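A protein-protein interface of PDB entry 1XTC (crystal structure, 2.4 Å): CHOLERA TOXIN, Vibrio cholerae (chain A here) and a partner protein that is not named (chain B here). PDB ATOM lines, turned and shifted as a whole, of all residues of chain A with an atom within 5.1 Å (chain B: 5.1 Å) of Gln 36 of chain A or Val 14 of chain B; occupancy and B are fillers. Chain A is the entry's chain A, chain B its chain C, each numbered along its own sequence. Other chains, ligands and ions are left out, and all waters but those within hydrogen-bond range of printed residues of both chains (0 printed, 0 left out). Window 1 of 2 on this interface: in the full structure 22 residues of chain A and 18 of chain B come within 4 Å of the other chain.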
ATOM      1  N   ASP A  32      -1.832  31.297   3.473  1.00  0.00           N
ATOM      2  CA  ASP A  32      -0.907  31.319   2.311  1.00  0.00           C
ATOM      3  C   ASP A  32       0.430  30.644   2.616  1.00  0.00           C
ATOM      4  O   ASP A  32       1.287  31.341   3.217  1.00  0.00           O
ATOM      5  CB  ASP A  32      -0.598  32.807   1.971  1.00  0.00           C
ATOM      6  CG  ASP A  32      -1.828  33.375   1.285  1.00  0.00           C
ATOM      7  OD1 ASP A  32      -2.106  32.906   0.166  1.00  0.00           O
ATOM      8  OD2 ASP A  32      -2.553  34.010   2.070  1.00  0.00           O
ATOM      9  N   ARG A  33       0.672  29.498   2.008  1.00  0.00           N
ATOM     10  CA  ARG A  33       1.974  28.812   2.256  1.00  0.00           C
ATOM     11  C   ARG A  33       3.003  29.398   1.290  1.00  0.00           C
ATOM     12  O   ARG A  33       4.217  29.403   1.574  1.00  0.00           O
ATOM     13  CB  ARG A  33       1.868  27.293   2.210  1.00  0.00           C
ATOM     14  CG  ARG A  33       1.568  26.706   3.606  1.00  0.00           C
ATOM     15  CD  ARG A  33       1.156  25.281   3.564  1.00  0.00           C
ATOM     16  NE  ARG A  33       0.268  24.966   4.680  1.00  0.00           N
ATOM     17  CZ  ARG A  33      -0.109  23.735   5.008  1.00  0.00           C
ATOM     18  NH1 ARG A  33       0.327  22.677   4.340  1.00  0.00           N
ATOM     19  NH2 ARG A  33      -0.981  23.541   5.998  1.00  0.00           N
ATOM     20  N   GLY A  34       2.405  29.970   0.269  1.00  0.00           N
ATOM     21  CA  GLY A  34       3.013  30.653  -0.866  1.00  0.00           C
ATOM     22  C   GLY A  34       2.459  32.098  -0.860  1.00  0.00           C
ATOM     23  O   GLY A  34       1.456  32.482  -1.462  1.00  0.00           O
ATOM     24  N   THR A  35       3.018  32.812   0.061  1.00  0.00           N
ATOM     25  CA  THR A  35       2.822  34.210   0.426  1.00  0.00           C
ATOM     26  C   THR A  35       3.725  34.264   1.695  1.00  0.00           C
ATOM     27  O   THR A  35       3.269  33.721   2.720  1.00  0.00           O
ATOM     28  CB  THR A  35       1.356  34.595   0.812  1.00  0.00           C
ATOM     29  OG1 THR A  35       0.806  35.365  -0.302  1.00  0.00           O
ATOM     30  CG2 THR A  35       1.250  35.407   2.119  1.00  0.00           C
ATOM     31  N   GLN A  36       5.014  34.334   1.345  1.00  0.00           N
ATOM     32  CA  GLN A  36       5.965  34.203   2.475  1.00  0.00           C
ATOM     33  C   GLN A  36       6.537  35.527   2.920  1.00  0.00           C
ATOM     34  O   GLN A  36       6.678  36.504   2.166  1.00  0.00           O
ATOM     35  CB  GLN A  36       6.926  33.045   2.389  1.00  0.00           C
ATOM     36  CG  GLN A  36       7.072  32.263   3.691  1.00  0.00           C
ATOM     37  CD  GLN A  36       5.764  32.039   4.418  1.00  0.00           C
ATOM     38  OE1 GLN A  36       5.603  32.359   5.604  1.00  0.00           O
ATOM     39  NE2 GLN A  36       4.765  31.563   3.662  1.00  0.00           N
ATOM     40  N   MET A  37       6.529  35.642   4.258  1.00  0.00           N
ATOM     41  CA  MET A  37       7.156  36.833   4.886  1.00  0.00           C
ATOM     42  C   MET A  37       8.487  36.280   5.478  1.00  0.00           C
ATOM     43  O   MET A  37       8.744  35.084   5.366  1.00  0.00           O
ATOM     44  CB  MET A  37       6.287  37.318   6.033  1.00  0.00           C
ATOM     45  CG  MET A  37       4.839  37.014   5.756  1.00  0.00           C
ATOM     46  SD  MET A  37       4.118  36.473   7.321  1.00  0.00           S
ATOM     47  CE  MET A  37       4.821  34.812   7.423  1.00  0.00           C
ATOM     48  N   ASN A  38       9.221  37.270   5.969  1.00  0.00           N
ATOM     49  CA  ASN A  38      10.420  36.957   6.761  1.00  0.00           C
ATOM     50  C   ASN A  38       9.876  36.468   8.130  1.00  0.00           C
ATOM     51  O   ASN A  38       8.925  37.039   8.677  1.00  0.00           O
ATOM     52  CB  ASN A  38      11.432  38.083   6.860  1.00  0.00           C
ATOM     53  CG  ASN A  38      12.755  37.573   7.454  1.00  0.00           C
ATOM     54  OD1 ASN A  38      12.767  36.593   8.234  1.00  0.00           O
ATOM     55  ND2 ASN A  38      13.876  38.022   6.877  1.00  0.00           N
ATOM     56  N   ILE A  39      10.384  35.323   8.519  1.00  0.00           N
ATOM     57  CA  ILE A  39      10.051  34.736   9.830  1.00  0.00           C
ATOM     58  C   ILE A  39      11.300  34.755  10.705  1.00  0.00           C
ATOM     59  O   ILE A  39      12.209  33.915  10.523  1.00  0.00           O
ATOM     60  CB  ILE A  39       9.354  33.361   9.669  1.00  0.00           C
ATOM     61  CG1 ILE A  39       8.123  33.591   8.714  1.00  0.00           C
ATOM     62  CG2 ILE A  39       8.925  32.719  11.009  1.00  0.00           C
ATOM     63  CD1 ILE A  39       7.284  32.291   8.535  1.00  0.00           C
ATOM     64  N   THR B   9      17.132  29.491   8.821  1.00  0.00           N
ATOM     65  CA  THR B   9      16.117  29.956   9.803  1.00  0.00           C
ATOM     66  C   THR B   9      14.688  29.885   9.207  1.00  0.00           C
ATOM     67  O   THR B   9      13.730  29.435   9.868  1.00  0.00           O
ATOM     68  CB  THR B   9      16.428  31.411  10.149  1.00  0.00           C
ATOM     69  OG1 THR B   9      17.836  31.611  10.092  1.00  0.00           O
ATOM     70  CG2 THR B   9      15.948  31.820  11.537  1.00  0.00           C
ATOM     71  N   GLN B  10      14.612  30.402   8.003  1.00  0.00           N
ATOM     72  CA  GLN B  10      13.413  30.424   7.152  1.00  0.00           C
ATOM     73  C   GLN B  10      12.959  29.007   6.794  1.00  0.00           C
ATOM     74  O   GLN B  10      11.779  28.647   6.923  1.00  0.00           O
ATOM     75  CB  GLN B  10      13.733  31.258   5.935  1.00  0.00           C
ATOM     76  CG  GLN B  10      14.526  32.506   6.337  1.00  0.00           C
ATOM     77  CD  GLN B  10      13.656  33.545   7.039  1.00  0.00           C
ATOM     78  OE1 GLN B  10      12.521  33.762   6.614  1.00  0.00           O
ATOM     79  NE2 GLN B  10      14.119  34.209   8.081  1.00  0.00           N
ATOM     80  N   SER B  11      13.904  28.192   6.373  1.00  0.00           N
ATOM     81  CA  SER B  11      13.556  26.840   5.985  1.00  0.00           C
ATOM     82  C   SER B  11      12.737  26.328   7.159  1.00  0.00           C
ATOM     83  O   SER B  11      11.617  25.829   6.969  1.00  0.00           O
ATOM     84  CB  SER B  11      14.871  26.048   5.761  1.00  0.00           C
ATOM     85  OG  SER B  11      14.708  24.673   6.079  1.00  0.00           O
ATOM     86  N   LEU B  12      13.356  26.570   8.296  1.00  0.00           N
ATOM     87  CA  LEU B  12      12.892  26.213   9.650  1.00  0.00           C
ATOM     88  C   LEU B  12      11.558  26.874  10.108  1.00  0.00           C
ATOM     89  O   LEU B  12      10.652  26.184  10.605  1.00  0.00           O
ATOM     90  CB  LEU B  12      13.974  26.634  10.641  1.00  0.00           C
ATOM     91  CG  LEU B  12      15.193  25.713  10.597  1.00  0.00           C
ATOM     92  CD1 LEU B  12      16.236  26.072  11.653  1.00  0.00           C
ATOM     93  CD2 LEU B  12      14.817  24.252  10.842  1.00  0.00           C
ATOM     94  N   GLY B  13      11.489  28.193   9.977  1.00  0.00           N
ATOM     95  CA  GLY B  13      10.304  29.031  10.341  1.00  0.00           C
ATOM     96  C   GLY B  13       9.043  28.660   9.529  1.00  0.00           C
ATOM     97  O   GLY B  13       7.925  28.594  10.065  1.00  0.00           O
ATOM     98  N   VAL B  14       9.250  28.510   8.228  1.00  0.00           N
ATOM     99  CA  VAL B  14       8.196  28.101   7.273  1.00  0.00           C
ATOM    100  C   VAL B  14       7.667  26.700   7.618  1.00  0.00           C
ATOM    101  O   VAL B  14       6.448  26.466   7.673  1.00  0.00           O
ATOM    102  CB  VAL B  14       8.737  28.166   5.852  1.00  0.00           C
ATOM    103  CG1 VAL B  14       7.885  27.388   4.853  1.00  0.00           C
ATOM    104  CG2 VAL B  14       8.797  29.607   5.328  1.00  0.00           C
ATOM    105  N   LYS B  15       8.621  25.824   7.841  1.00  0.00           N
ATOM    106  CA  LYS B  15       8.370  24.436   8.209  1.00  0.00           C
ATOM    107  C   LYS B  15       7.485  24.438   9.456  1.00  0.00           C
ATOM    108  O   LYS B  15       6.426  23.797   9.498  1.00  0.00           O
ATOM    109  CB  LYS B  15       9.745  23.815   8.502  1.00  0.00           C
ATOM    110  CG  LYS B  15       9.740  22.360   8.955  1.00  0.00           C
ATOM    111  CD  LYS B  15      11.128  21.904   9.439  1.00  0.00           C
ATOM    112  CE  LYS B  15      11.102  21.352  10.863  1.00  0.00           C
ATOM    113  NZ  LYS B  15      12.443  21.132  11.419  1.00  0.00           N
ATOM    114  N   PHE B  16       7.916  25.212  10.443  1.00  0.00           N
ATOM    115  CA  PHE B  16       7.181  25.296  11.707  1.00  0.00           C
ATOM    116  C   PHE B  16       5.741  25.775  11.452  1.00  0.00           C
ATOM    117  O   PHE B  16       4.778  25.141  11.889  1.00  0.00           O
ATOM    118  CB  PHE B  16       7.861  26.265  12.690  1.00  0.00           C
ATOM    119  CG  PHE B  16       7.056  26.417  13.987  1.00  0.00           C
ATOM    120  CD1 PHE B  16       7.288  25.561  15.074  1.00  0.00           C
ATOM    121  CD2 PHE B  16       6.074  27.410  14.085  1.00  0.00           C
ATOM    122  CE1 PHE B  16       6.503  25.661  16.228  1.00  0.00           C
ATOM    123  CE2 PHE B  16       5.301  27.522  15.247  1.00  0.00           C
ATOM    124  CZ  PHE B  16       5.508  26.641  16.314  1.00  0.00           C
ATOM    125  N   LEU B  17       5.622  26.873  10.721  1.00  0.00           N
ATOM    126  CA  LEU B  17       4.314  27.505  10.394  1.00  0.00           C
ATOM    127  C   LEU B  17       3.384  26.522   9.646  1.00  0.00           C
ATOM    128  O   LEU B  17       2.166  26.498   9.861  1.00  0.00           O
ATOM    129  CB  LEU B  17       4.513  28.789   9.575  1.00  0.00           C
ATOM    130  CG  LEU B  17       3.206  29.565   9.309  1.00  0.00           C
ATOM    131  CD1 LEU B  17       2.361  29.834  10.560  1.00  0.00           C
ATOM    132  CD2 LEU B  17       3.448  30.943   8.677  1.00  0.00           C
ATOM    133  N   ASP B  18       3.950  25.758   8.727  1.00  0.00           N
ATOM    134  CA  ASP B  18       3.174  24.795   7.911  1.00  0.00           C
ATOM    135  C   ASP B  18       2.433  23.702   8.745  1.00  0.00           C
ATOM    136  O   ASP B  18       1.211  23.516   8.593  1.00  0.00           O
ATOM    137  CB  ASP B  18       4.103  24.218   6.859  1.00  0.00           C
ATOM    138  CG  ASP B  18       4.439  25.313   5.857  1.00  0.00           C
ATOM    139  OD1 ASP B  18       3.760  26.416   5.890  1.00  0.00           O
ATOM    140  OD2 ASP B  18       5.373  25.155   4.996  1.00  0.00           O
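Printed residues of chain B that touch a printed residue of chain A: Gln 10, Gly 13, Val 14 and Asp 18.
Of the 8 printed residues of chain A, 4 touch a printed residue of chain B.
Among the printed residues, Asp or Glu carboxylates within 4 Å of a Lys or Arg side-chain nitrogen of the other chain: Arg 33 of chain A with Asp 18 of chain B (3.97 Å).
The side-chain carboxylate (OD1) of Asp 18 of chain B lies within salt-bridge range of the guanidinium group (NE) of Arg 33 of chain A.
The side-chain amide nitrogen of Gln 10 of chain B sits at hydrogen-bond distance from the side-chain amide oxygen of Asn 38 of chain A, 2.7 Å away.
The backbone carbonyl oxygen (O) of Ile 39 of chain A is in hydrogen-bond range of the side-chain amide nitrogen (NE2) of Gln 10 of chain B (3.1 Å).
Of the printed residues of chain B, Arg 33 of chain A touches Asp 18 (3.2 Å).
Of the printed residues of chain B, Gln 36 of chain A touches Val 14 (3.6 Å).
Of the printed residues of chain B, Asn 38 of chain A touches Gln 10 (2.7 Å).
Of the printed residues of chain B, Ile 39 of chain A touches Gln 10 and Gly 13.
Printed residues of chain A within 4 Å of Gln 10 of chain B: Asn 38 (2.7 Å) and Ile 39 (3.1 Å).
Of chain A, only Gln 36 (3.6 Å) comes within 4 Å of Val 14 of chain B.
Printed residues of chain A within 4 Å of Asp 18 of chain B: Arg 33 (3.2 Å).
The nearest printed residue of chain B that does not touch Gln 36 of chain A is Leu 17 of chain B (4.01 Å).
The side-chain amide nitrogen of Gln 36 of chain A sits at hydrogen-bond distance from the backbone carbonyl oxygen of Arg 33 of chain A, at 3.1 Å.
Among the printed residues, pairs that only touch across the chains: Gln 36 of chain A with Val 14 of chain B (3.6 Å) and Ile 39 of chain A with Gly 13 of chain B (3.99 Å).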
